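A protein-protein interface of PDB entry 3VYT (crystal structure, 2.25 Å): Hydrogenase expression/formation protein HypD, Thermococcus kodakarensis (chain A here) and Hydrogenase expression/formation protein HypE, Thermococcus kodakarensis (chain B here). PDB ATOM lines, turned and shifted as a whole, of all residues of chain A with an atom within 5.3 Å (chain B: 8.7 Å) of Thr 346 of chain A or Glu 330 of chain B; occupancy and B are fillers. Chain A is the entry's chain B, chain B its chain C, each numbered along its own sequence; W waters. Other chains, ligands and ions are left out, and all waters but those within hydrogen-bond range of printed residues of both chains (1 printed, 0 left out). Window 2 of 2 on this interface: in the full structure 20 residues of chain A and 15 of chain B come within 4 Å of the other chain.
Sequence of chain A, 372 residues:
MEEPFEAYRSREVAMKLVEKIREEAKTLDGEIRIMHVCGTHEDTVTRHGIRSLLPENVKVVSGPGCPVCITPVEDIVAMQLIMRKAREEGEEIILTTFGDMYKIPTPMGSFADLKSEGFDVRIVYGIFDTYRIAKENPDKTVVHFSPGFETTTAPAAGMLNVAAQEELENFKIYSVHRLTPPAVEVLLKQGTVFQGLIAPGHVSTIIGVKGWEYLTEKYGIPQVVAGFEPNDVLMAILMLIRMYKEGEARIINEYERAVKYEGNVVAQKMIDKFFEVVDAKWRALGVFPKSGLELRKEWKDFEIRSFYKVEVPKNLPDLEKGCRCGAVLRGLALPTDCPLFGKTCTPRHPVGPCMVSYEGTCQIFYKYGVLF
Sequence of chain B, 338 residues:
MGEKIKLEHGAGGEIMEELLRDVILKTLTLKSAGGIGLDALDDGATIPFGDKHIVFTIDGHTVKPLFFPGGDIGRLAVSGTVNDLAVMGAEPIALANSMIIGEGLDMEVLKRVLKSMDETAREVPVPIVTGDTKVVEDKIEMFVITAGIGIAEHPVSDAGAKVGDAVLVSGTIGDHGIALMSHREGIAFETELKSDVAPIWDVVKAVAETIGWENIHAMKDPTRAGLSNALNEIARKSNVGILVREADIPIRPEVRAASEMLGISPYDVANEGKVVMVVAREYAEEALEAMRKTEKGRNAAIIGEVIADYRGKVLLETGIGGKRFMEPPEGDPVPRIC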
ATOM      1  N   GLY A 342      31.579  13.217  12.196  1.00  0.00           N
ATOM      2  CA  GLY A 342      31.887  14.432  11.462  1.00  0.00           C
ATOM      3  C   GLY A 342      32.676  14.214  10.191  1.00  0.00           C
ATOM      4  O   GLY A 342      33.032  15.165   9.500  1.00  0.00           O
ATOM      5  N   LYS A 343      32.968  12.959   9.883  1.00  0.00           N
ATOM      6  CA  LYS A 343      33.702  12.635   8.676  1.00  0.00           C
ATOM      7  C   LYS A 343      32.679  12.066   7.694  1.00  0.00           C
ATOM      8  O   LYS A 343      31.960  12.824   7.045  1.00  0.00           O
ATOM      9  CB  LYS A 343      34.801  11.622   8.979  1.00  0.00           C
ATOM     10  N   THR A 344      32.595  10.746   7.581  1.00  0.00           N
ATOM     11  CA  THR A 344      31.621  10.176   6.673  1.00  0.00           C
ATOM     12  C   THR A 344      30.250  10.168   7.328  1.00  0.00           C
ATOM     13  O   THR A 344      29.230   9.986   6.659  1.00  0.00           O
ATOM     14  CB  THR A 344      31.981   8.731   6.265  1.00  0.00           C
ATOM     15  OG1 THR A 344      32.307   7.972   7.429  1.00  0.00           O
ATOM     16  CG2 THR A 344      33.146   8.723   5.287  1.00  0.00           C
ATOM     17  N   CYS A 345      30.226  10.382   8.638  1.00  0.00           N
ATOM     18  CA  CYS A 345      28.965  10.380   9.359  1.00  0.00           C
ATOM     19  C   CYS A 345      28.561  11.758   9.859  1.00  0.00           C
ATOM     20  O   CYS A 345      29.259  12.372  10.666  1.00  0.00           O
ATOM     21  CB  CYS A 345      29.039   9.408  10.539  1.00  0.00           C
ATOM     22  SG  CYS A 345      27.415   9.001  11.253  1.00  0.00           S
ATOM     23  N   THR A 346      27.430  12.242   9.356  1.00  0.00           N
ATOM     24  CA  THR A 346      26.879  13.540   9.750  1.00  0.00           C
ATOM     25  C   THR A 346      25.371  13.372   9.669  1.00  0.00           C
ATOM     26  O   THR A 346      24.883  12.353   9.173  1.00  0.00           O
ATOM     27  CB  THR A 346      27.303  14.700   8.794  1.00  0.00           C
ATOM     28  OG1 THR A 346      26.865  14.415   7.459  1.00  0.00           O
ATOM     29  CG2 THR A 346      28.815  14.891   8.807  1.00  0.00           C
ATOM     30  N   PRO A 347      24.612  14.351  10.175  1.00  0.00           N
ATOM     31  CA  PRO A 347      23.154  14.278  10.139  1.00  0.00           C
ATOM     32  C   PRO A 347      22.626  14.147   8.724  1.00  0.00           C
ATOM     33  O   PRO A 347      21.661  13.427   8.483  1.00  0.00           O
ATOM     34  CB  PRO A 347      22.736  15.587  10.791  1.00  0.00           C
ATOM     35  CG  PRO A 347      23.803  15.790  11.801  1.00  0.00           C
ATOM     36  CD  PRO A 347      25.054  15.474  11.017  1.00  0.00           C
ATOM     37  N   ARG A 348      23.269  14.842   7.790  1.00  0.00           N
ATOM     38  CA  ARG A 348      22.854  14.804   6.396  1.00  0.00           C
ATOM     39  C   ARG A 348      23.114  13.446   5.766  1.00  0.00           C
ATOM     40  O   ARG A 348      22.268  12.924   5.045  1.00  0.00           O
ATOM     41  CB  ARG A 348      23.571  15.897   5.599  1.00  0.00           C
ATOM     42  CG  ARG A 348      22.838  17.233   5.571  1.00  0.00           C
ATOM     43  CD  ARG A 348      21.461  17.094   4.923  1.00  0.00           C
ATOM     44  NE  ARG A 348      20.375  17.056   5.900  1.00  0.00           N
ATOM     45  CZ  ARG A 348      19.922  18.120   6.558  1.00  0.00           C
ATOM     46  NH1 ARG A 348      20.457  19.314   6.345  1.00  0.00           N
ATOM     47  NH2 ARG A 348      18.932  17.989   7.430  1.00  0.00           N
ATOM     48  N   HIS A 349      24.286  12.881   6.033  1.00  0.00           N
ATOM     49  CA  HIS A 349      24.640  11.569   5.499  1.00  0.00           C
ATOM     50  C   HIS A 349      25.160  10.692   6.631  1.00  0.00           C
ATOM     51  O   HIS A 349      26.364  10.451   6.764  1.00  0.00           O
ATOM     52  CB  HIS A 349      25.667  11.690   4.360  1.00  0.00           C
ATOM     53  CG  HIS A 349      26.898  12.470   4.708  1.00  0.00           C
ATOM     54  ND1 HIS A 349      27.976  11.910   5.360  1.00  0.00           N
ATOM     55  CD2 HIS A 349      27.239  13.757   4.455  1.00  0.00           C
ATOM     56  CE1 HIS A 349      28.929  12.815   5.488  1.00  0.00           C
ATOM     57  NE2 HIS A 349      28.508  13.944   4.947  1.00  0.00           N
ATOM     58  N   PRO A 350      24.234  10.203   7.473  1.00  0.00           N
ATOM     59  CA  PRO A 350      24.514   9.348   8.631  1.00  0.00           C
ATOM     60  C   PRO A 350      24.937   7.921   8.327  1.00  0.00           C
ATOM     61  O   PRO A 350      24.444   7.289   7.395  1.00  0.00           O
ATOM     62  CB  PRO A 350      23.204   9.389   9.414  1.00  0.00           C
ATOM     63  CG  PRO A 350      22.177   9.477   8.322  1.00  0.00           C
ATOM     64  CD  PRO A 350      22.788  10.494   7.372  1.00  0.00           C
ATOM     65  N   VAL A 351      25.860   7.422   9.138  1.00  0.00           N
ATOM     66  CA  VAL A 351      26.330   6.066   9.000  1.00  0.00           C
ATOM     67  C   VAL A 351      25.618   5.214  10.051  1.00  0.00           C
ATOM     68  O   VAL A 351      25.208   4.090   9.772  1.00  0.00           O
ATOM     69  CB  VAL A 351      27.839   5.977   9.223  1.00  0.00           C
ATOM     70  CG1 VAL A 351      28.293   4.530   9.055  1.00  0.00           C
ATOM     71  CG2 VAL A 351      28.566   6.886   8.220  1.00  0.00           C
ATOM     72  N   MET A 355      23.355   9.134  14.895  1.00  0.00           N
ATOM     73  CA  MET A 355      23.522  10.403  14.185  1.00  0.00           C
ATOM     74  C   MET A 355      22.223  10.821  13.488  1.00  0.00           C
ATOM     75  O   MET A 355      21.931  12.007  13.356  1.00  0.00           O
ATOM     76  CB  MET A 355      24.663  10.279  13.160  1.00  0.00           C
ATOM     77  CG  MET A 355      25.015  11.567  12.401  1.00  0.00           C
ATOM     78  SD  MET A 355      25.585  12.913  13.474  1.00  0.00           S
ATOM     79  CE  MET A 355      27.294  12.478  13.674  1.00  0.00           C
ATOM     80  N   TYR A 366      27.022  16.716  17.180  1.00  0.00           N
ATOM     81  CA  TYR A 366      27.334  17.314  15.892  1.00  0.00           C
ATOM     82  C   TYR A 366      26.654  18.676  15.690  1.00  0.00           C
ATOM     83  O   TYR A 366      27.280  19.678  15.325  1.00  0.00           O
ATOM     84  CB  TYR A 366      26.889  16.384  14.767  1.00  0.00           C
ATOM     85  CG  TYR A 366      27.320  16.885  13.421  1.00  0.00           C
ATOM     86  CD1 TYR A 366      28.604  16.632  12.944  1.00  0.00           C
ATOM     87  CD2 TYR A 366      26.478  17.679  12.652  1.00  0.00           C
ATOM     88  CE1 TYR A 366      29.037  17.158  11.744  1.00  0.00           C
ATOM     89  CE2 TYR A 366      26.904  18.209  11.444  1.00  0.00           C
ATOM     90  CZ  TYR A 366      28.185  17.945  10.996  1.00  0.00           C
ATOM     91  OH  TYR A 366      28.615  18.471   9.801  1.00  0.00           O
ATOM     92  N   LEU B   7      20.371  17.964  -2.836  1.00  0.00           N
ATOM     93  CA  LEU B   7      19.705  19.180  -2.381  1.00  0.00           C
ATOM     94  C   LEU B   7      20.657  19.986  -1.496  1.00  0.00           C
ATOM     95  O   LEU B   7      20.639  21.219  -1.495  1.00  0.00           O
ATOM     96  CB  LEU B   7      18.449  18.802  -1.588  1.00  0.00           C
ATOM     97  CG  LEU B   7      17.061  19.177  -2.115  1.00  0.00           C
ATOM     98  CD1 LEU B   7      17.057  19.318  -3.634  1.00  0.00           C
ATOM     99  CD2 LEU B   7      16.075  18.106  -1.671  1.00  0.00           C
ATOM    100  N   GLU B   8      21.490  19.269  -0.747  1.00  0.00           N
ATOM    101  CA  GLU B   8      22.472  19.866   0.160  1.00  0.00           C
ATOM    102  C   GLU B   8      23.506  20.716  -0.566  1.00  0.00           C
ATOM    103  O   GLU B   8      24.030  21.680  -0.010  1.00  0.00           O
ATOM    104  CB  GLU B   8      23.218  18.770   0.928  1.00  0.00           C
ATOM    105  CG  GLU B   8      22.392  18.021   1.947  1.00  0.00           C
ATOM    106  CD  GLU B   8      21.199  17.316   1.343  1.00  0.00           C
ATOM    107  OE1 GLU B   8      21.390  16.492   0.424  1.00  0.00           O
ATOM    108  OE2 GLU B   8      20.065  17.588   1.790  1.00  0.00           O
ATOM    109  N   HIS B   9      23.818  20.352  -1.802  1.00  0.00           N
ATOM    110  CA  HIS B   9      24.816  21.091  -2.555  1.00  0.00           C
ATOM    111  C   HIS B   9      24.398  22.522  -2.889  1.00  0.00           C
ATOM    112  O   HIS B   9      25.222  23.329  -3.329  1.00  0.00           O
ATOM    113  CB  HIS B   9      25.189  20.318  -3.821  1.00  0.00           C
ATOM    114  CG  HIS B   9      25.925  19.042  -3.543  1.00  0.00           C
ATOM    115  ND1 HIS B   9      25.283  17.834  -3.368  1.00  0.00           N
ATOM    116  CD2 HIS B   9      27.244  18.797  -3.356  1.00  0.00           C
ATOM    117  CE1 HIS B   9      26.176  16.902  -3.084  1.00  0.00           C
ATOM    118  NE2 HIS B   9      27.373  17.460  -3.070  1.00  0.00           N
ATOM    119  N   GLY B  10      23.124  22.839  -2.668  1.00  0.00           N
ATOM    120  CA  GLY B  10      22.651  24.187  -2.939  1.00  0.00           C
ATOM    121  C   GLY B  10      21.952  24.793  -1.735  1.00  0.00           C
ATOM    122  O   GLY B  10      21.133  25.701  -1.878  1.00  0.00           O
ATOM    123  N   ALA B  11      22.285  24.303  -0.542  1.00  0.00           N
ATOM    124  CA  ALA B  11      21.654  24.792   0.683  1.00  0.00           C
ATOM    125  C   ALA B  11      22.456  25.859   1.439  1.00  0.00           C
ATOM    126  O   ALA B  11      22.124  26.200   2.576  1.00  0.00           O
ATOM    127  CB  ALA B  11      21.337  23.614   1.606  1.00  0.00           C
ATOM    128  N   GLY B  12      23.509  26.376   0.806  1.00  0.00           N
ATOM    129  CA  GLY B  12      24.325  27.416   1.409  1.00  0.00           C
ATOM    130  C   GLY B  12      25.122  27.053   2.649  1.00  0.00           C
ATOM    131  O   GLY B  12      25.711  27.930   3.289  1.00  0.00           O
ATOM    132  N   GLY B  13      25.150  25.772   3.000  1.00  0.00           N
ATOM    133  CA  GLY B  13      25.897  25.359   4.170  1.00  0.00           C
ATOM    134  C   GLY B  13      27.304  24.881   3.849  1.00  0.00           C
ATOM    135  O   GLY B  13      27.967  25.410   2.949  1.00  0.00           O
ATOM    136  N   GLU B  14      27.747  23.868   4.595  1.00  0.00           N
ATOM    137  CA  GLU B  14      29.074  23.272   4.449  1.00  0.00           C
ATOM    138  C   GLU B  14      29.166  22.376   3.216  1.00  0.00           C
ATOM    139  O   GLU B  14      30.136  22.442   2.458  1.00  0.00           O
ATOM    140  CB  GLU B  14      29.418  22.463   5.717  1.00  0.00           C
ATOM    141  N   ILE B  15      28.155  21.536   3.026  1.00  0.00           N
ATOM    142  CA  ILE B  15      28.112  20.630   1.884  1.00  0.00           C
ATOM    143  C   ILE B  15      28.207  21.432   0.583  1.00  0.00           C
ATOM    144  O   ILE B  15      28.846  20.992  -0.372  1.00  0.00           O
ATOM    145  CB  ILE B  15      26.811  19.780   1.907  1.00  0.00           C
ATOM    146  CG1 ILE B  15      26.824  18.870   3.141  1.00  0.00           C
ATOM    147  CG2 ILE B  15      26.692  18.952   0.630  1.00  0.00           C
ATOM    148  CD1 ILE B  15      25.577  18.026   3.322  1.00  0.00           C
ATOM    149  N   MET B  16      27.584  22.611   0.549  1.00  0.00           N
ATOM    150  CA  MET B  16      27.647  23.448  -0.645  1.00  0.00           C
ATOM    151  C   MET B  16      29.039  24.040  -0.764  1.00  0.00           C
ATOM    152  O   MET B  16      29.514  24.325  -1.858  1.00  0.00           O
ATOM    153  CB  MET B  16      26.620  24.585  -0.592  1.00  0.00           C
ATOM    154  CG  MET B  16      26.749  25.568  -1.766  1.00  0.00           C
ATOM    155  SD  MET B  16      25.306  26.618  -2.056  1.00  0.00           S
ATOM    156  CE  MET B  16      25.866  28.173  -1.427  1.00  0.00           C
ATOM    157  N   GLU B  17      29.689  24.228   0.376  1.00  0.00           N
ATOM    158  CA  GLU B  17      31.032  24.780   0.391  1.00  0.00           C
ATOM    159  C   GLU B  17      31.945  23.755  -0.258  1.00  0.00           C
ATOM    160  O   GLU B  17      32.882  24.102  -0.975  1.00  0.00           O
ATOM    161  CB  GLU B  17      31.485  25.039   1.829  1.00  0.00           C
ATOM    162  CG  GLU B  17      32.576  26.080   1.948  1.00  0.00           C
ATOM    163  CD  GLU B  17      32.116  27.432   1.445  1.00  0.00           C
ATOM    164  OE1 GLU B  17      31.097  27.940   1.961  1.00  0.00           O
ATOM    165  OE2 GLU B  17      32.768  27.984   0.535  1.00  0.00           O
ATOM    166  N   GLU B  18      31.658  22.484   0.002  1.00  0.00           N
ATOM    167  CA  GLU B  18      32.451  21.403  -0.565  1.00  0.00           C
ATOM    168  C   GLU B  18      32.358  21.463  -2.091  1.00  0.00           C
ATOM    169  O   GLU B  18      33.381  21.454  -2.782  1.00  0.00           O
ATOM    170  CB  GLU B  18      31.944  20.044  -0.069  1.00  0.00           C
ATOM    171  CG  GLU B  18      31.716  19.970   1.426  1.00  0.00           C
ATOM    172  CD  GLU B  18      31.343  18.573   1.890  1.00  0.00           C
ATOM    173  OE1 GLU B  18      30.752  18.445   2.981  1.00  0.00           O
ATOM    174  OE2 GLU B  18      31.651  17.602   1.170  1.00  0.00           O
ATOM    175  N   ALA B 225      21.451  29.421   5.275  1.00  0.00           N
ATOM    176  CA  ALA B 225      22.264  28.878   6.347  1.00  0.00           C
ATOM    177  C   ALA B 225      22.318  29.786   7.571  1.00  0.00           C
ATOM    178  O   ALA B 225      22.958  29.462   8.551  1.00  0.00           O
ATOM    179  CB  ALA B 225      23.652  28.545   5.850  1.00  0.00           C
ATOM    180  N   SER B 228      24.440  31.829  11.933  1.00  0.00           N
ATOM    181  CA  SER B 228      25.580  30.968  12.205  1.00  0.00           C
ATOM    182  C   SER B 228      26.483  30.894  10.975  1.00  0.00           C
ATOM    183  O   SER B 228      27.687  31.098  11.071  1.00  0.00           O
ATOM    184  CB  SER B 228      25.108  29.566  12.603  1.00  0.00           C
ATOM    185  OG  SER B 228      24.373  28.966  11.559  1.00  0.00           O
ATOM    186  N   ASN B 229      25.903  30.633   9.811  1.00  0.00           N
ATOM    187  CA  ASN B 229      26.707  30.550   8.598  1.00  0.00           C
ATOM    188  C   ASN B 229      27.398  31.863   8.237  1.00  0.00           C
ATOM    189  O   ASN B 229      28.576  31.868   7.899  1.00  0.00           O
ATOM    190  CB  ASN B 229      25.863  30.104   7.405  1.00  0.00           C
ATOM    191  CG  ASN B 229      26.618  30.226   6.101  1.00  0.00           C
ATOM    192  OD1 ASN B 229      27.374  29.333   5.716  1.00  0.00           O
ATOM    193  ND2 ASN B 229      26.441  31.353   5.427  1.00  0.00           N
ATOM    194  N   ASP B 268      20.277  28.928  12.134  1.00  0.00           N
ATOM    195  CA  ASP B 268      20.678  28.240  10.908  1.00  0.00           C
ATOM    196  C   ASP B 268      19.780  28.484   9.693  1.00  0.00           C
ATOM    197  O   ASP B 268      20.043  27.950   8.615  1.00  0.00           O
ATOM    198  CB  ASP B 268      20.776  26.718  11.154  1.00  0.00           C
ATOM    199  CG  ASP B 268      21.513  26.350  12.460  1.00  0.00           C
ATOM    200  OD1 ASP B 268      22.579  26.924  12.774  1.00  0.00           O
ATOM    201  OD2 ASP B 268      21.021  25.450  13.176  1.00  0.00           O
ATOM    202  N   GLU B 327      27.951  26.062  15.371  1.00  0.00           N
ATOM    203  CA  GLU B 327      28.282  25.360  14.147  1.00  0.00           C
ATOM    204  C   GLU B 327      27.578  25.821  12.882  1.00  0.00           C
ATOM    205  O   GLU B 327      26.367  26.053  12.870  1.00  0.00           O
ATOM    206  CB  GLU B 327      28.049  23.865  14.345  1.00  0.00           C
ATOM    207  CG  GLU B 327      29.092  23.207  15.228  1.00  0.00           C
ATOM    208  CD  GLU B 327      30.494  23.349  14.655  1.00  0.00           C
ATOM    209  OE1 GLU B 327      30.712  22.898  13.508  1.00  0.00           O
ATOM    210  OE2 GLU B 327      31.373  23.911  15.345  1.00  0.00           O
ATOM    211  N   PRO B 328      28.343  25.981  11.795  1.00  0.00           N
ATOM    212  CA  PRO B 328      27.770  26.410  10.519  1.00  0.00           C
ATOM    213  C   PRO B 328      26.981  25.210  10.004  1.00  0.00           C
ATOM    214  O   PRO B 328      27.550  24.147   9.793  1.00  0.00           O
ATOM    215  CB  PRO B 328      29.006  26.712   9.674  1.00  0.00           C
ATOM    216  CG  PRO B 328      30.011  25.722  10.190  1.00  0.00           C
ATOM    217  CD  PRO B 328      29.799  25.773  11.682  1.00  0.00           C
ATOM    218  N   PRO B 329      25.667  25.359   9.805  1.00  0.00           N
ATOM    219  CA  PRO B 329      24.865  24.232   9.322  1.00  0.00           C
ATOM    220  C   PRO B 329      25.447  23.512   8.117  1.00  0.00           C
ATOM    221  O   PRO B 329      26.224  24.088   7.359  1.00  0.00           O
ATOM    222  CB  PRO B 329      23.513  24.872   9.025  1.00  0.00           C
ATOM    223  CG  PRO B 329      23.871  26.281   8.695  1.00  0.00           C
ATOM    224  CD  PRO B 329      24.898  26.612   9.737  1.00  0.00           C
ATOM    225  N   GLU B 330      25.098  22.238   7.970  1.00  0.00           N
ATOM    226  CA  GLU B 330      25.568  21.449   6.838  1.00  0.00           C
ATOM    227  C   GLU B 330      24.883  22.031   5.611  1.00  0.00           C
ATOM    228  O   GLU B 330      25.429  22.042   4.509  1.00  0.00           O
ATOM    229  CB  GLU B 330      25.174  19.974   6.996  1.00  0.00           C
ATOM    230  CG  GLU B 330      26.173  19.123   7.779  1.00  0.00           C
ATOM    231  CD  GLU B 330      25.913  17.622   7.615  1.00  0.00           C
ATOM    232  OE1 GLU B 330      24.939  17.096   8.211  1.00  0.00           O
ATOM    233  OE2 GLU B 330      26.681  16.971   6.873  1.00  0.00           O
ATOM    234  N   GLY B 331      23.676  22.526   5.832  1.00  0.00           N
ATOM    235  CA  GLY B 331      22.904  23.135   4.770  1.00  0.00           C
ATOM    236  C   GLY B 331      21.669  23.725   5.414  1.00  0.00           C
ATOM    237  O   GLY B 331      21.277  23.289   6.496  1.00  0.00           O
ATOM    238  N   ASP B 332      21.055  24.716   4.778  1.00  0.00           N
ATOM    239  CA  ASP B 332      19.853  25.307   5.349  1.00  0.00           C
ATOM    240  C   ASP B 332      18.840  24.182   5.598  1.00  0.00           C
ATOM    241  O   ASP B 332      18.596  23.340   4.732  1.00  0.00           O
ATOM    242  CB  ASP B 332      19.262  26.356   4.400  1.00  0.00           C
ATOM    243  CG  ASP B 332      18.322  27.329   5.112  1.00  0.00           C
ATOM    244  OD1 ASP B 332      17.371  26.867   5.787  1.00  0.00           O
ATOM    245  OD2 ASP B 332      18.538  28.556   4.996  1.00  0.00           O
ATOM    246  N   PRO B 333      18.249  24.152   6.795  1.00  0.00           N
ATOM    247  CA  PRO B 333      17.269  23.125   7.154  1.00  0.00           C
ATOM    248  C   PRO B 333      16.023  23.116   6.267  1.00  0.00           C
ATOM    249  O   PRO B 333      15.550  22.052   5.863  1.00  0.00           O
ATOM    250  CB  PRO B 333      16.927  23.467   8.605  1.00  0.00           C
ATOM    251  CG  PRO B 333      18.163  24.153   9.103  1.00  0.00           C
ATOM    252  CD  PRO B 333      18.524  25.036   7.939  1.00  0.00           C
HETATM  253  O   HOH W   1      29.249  17.052   5.415  1.00  0.00           O
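OE2 of Glu 330 of chain B lies within hydrogen-bond range of OG1 of Thr 346 of chain A.
The backbone NH of Arg 348 of chain A lies within hydrogen-bond range of the side-chain carboxylate of Glu 330 of chain B.
N of Pro 347 of chain A lies close to OE1 of Glu 330 of chain B (3.4 Å).
OG1 of Thr 346 of chain A sits at hydrogen-bond distance from NE2 of His 349 of chain A, at 3.0 Å.
N of Glu 14 of chain B lies within hydrogen-bond range of O of Glu 330 of chain B (3.0 Å).
O of Glu 330 of chain B is in hydrogen-bond range of N of Ile 15 of chain B, at 3.1 Å.
Arg 348 of chain A touches Glu 8 of chain B (CD to CG, 3.3 Å).
Ile 15 of chain B touches Arg 348 of chain A.
Tyr 366 of chain A touches Glu 327 of chain B (O to CG, 3.97 Å).
OH of Tyr 366 of chain A touches CG of Glu 330 of chain B, at 3.2 Å.
Of chain B, only Glu 330 (2.6 Å) comes within 4 Å of Thr 346 of chain A.
Of the printed residues of chain A, Glu 330 of chain B touches Thr 346 (2.6 Å), Pro 347 (3.2 Å), Arg 348 (2.8 Å) and Tyr 366 (3.2 Å).
No residue of chain B comes within 4 Å of His 349 of chain A.
Of the printed residues of chain B, Tyr 366 of chain A touches Glu 327 and Glu 330.
Of the printed residues of chain A, Glu 327 of chain B touches Tyr 366 (3.97 Å).
Printed residues of chain B within 4 Å of Arg 348 of chain A: Glu 8 (3.3 Å), Ile 15 (3.6 Å) and Glu 330 (2.8 Å).
Of the printed residues of chain A, Glu 8 of chain B touches Arg 348 (3.3 Å).
Leu 7 of chain B touches none of the printed residues of chain A.
Lys 343 of chain A touches none of the printed residues of chain B.
The nearest printed residue of chain A that does not touch Glu 330 of chain B is His 349 of chain A (4.03 Å).
Of the 23 printed residues of chain B, 4 touch a printed residue of chain A.
Hydrophobic or aromatic side chains of chain B that line the printed part of chain A: Ile 15.
Among the printed residues, 7 pairs touch across the chains.
Water W1 lies within hydrogen-bond range of the side-chain carboxylate of Glu 330 of chain B (3.0 Å), the side-chain carboxylate of Glu 18 of chain B (3.2 Å) and a ring nitrogen (NE2) of His 349 of chain A (3.2 Å).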
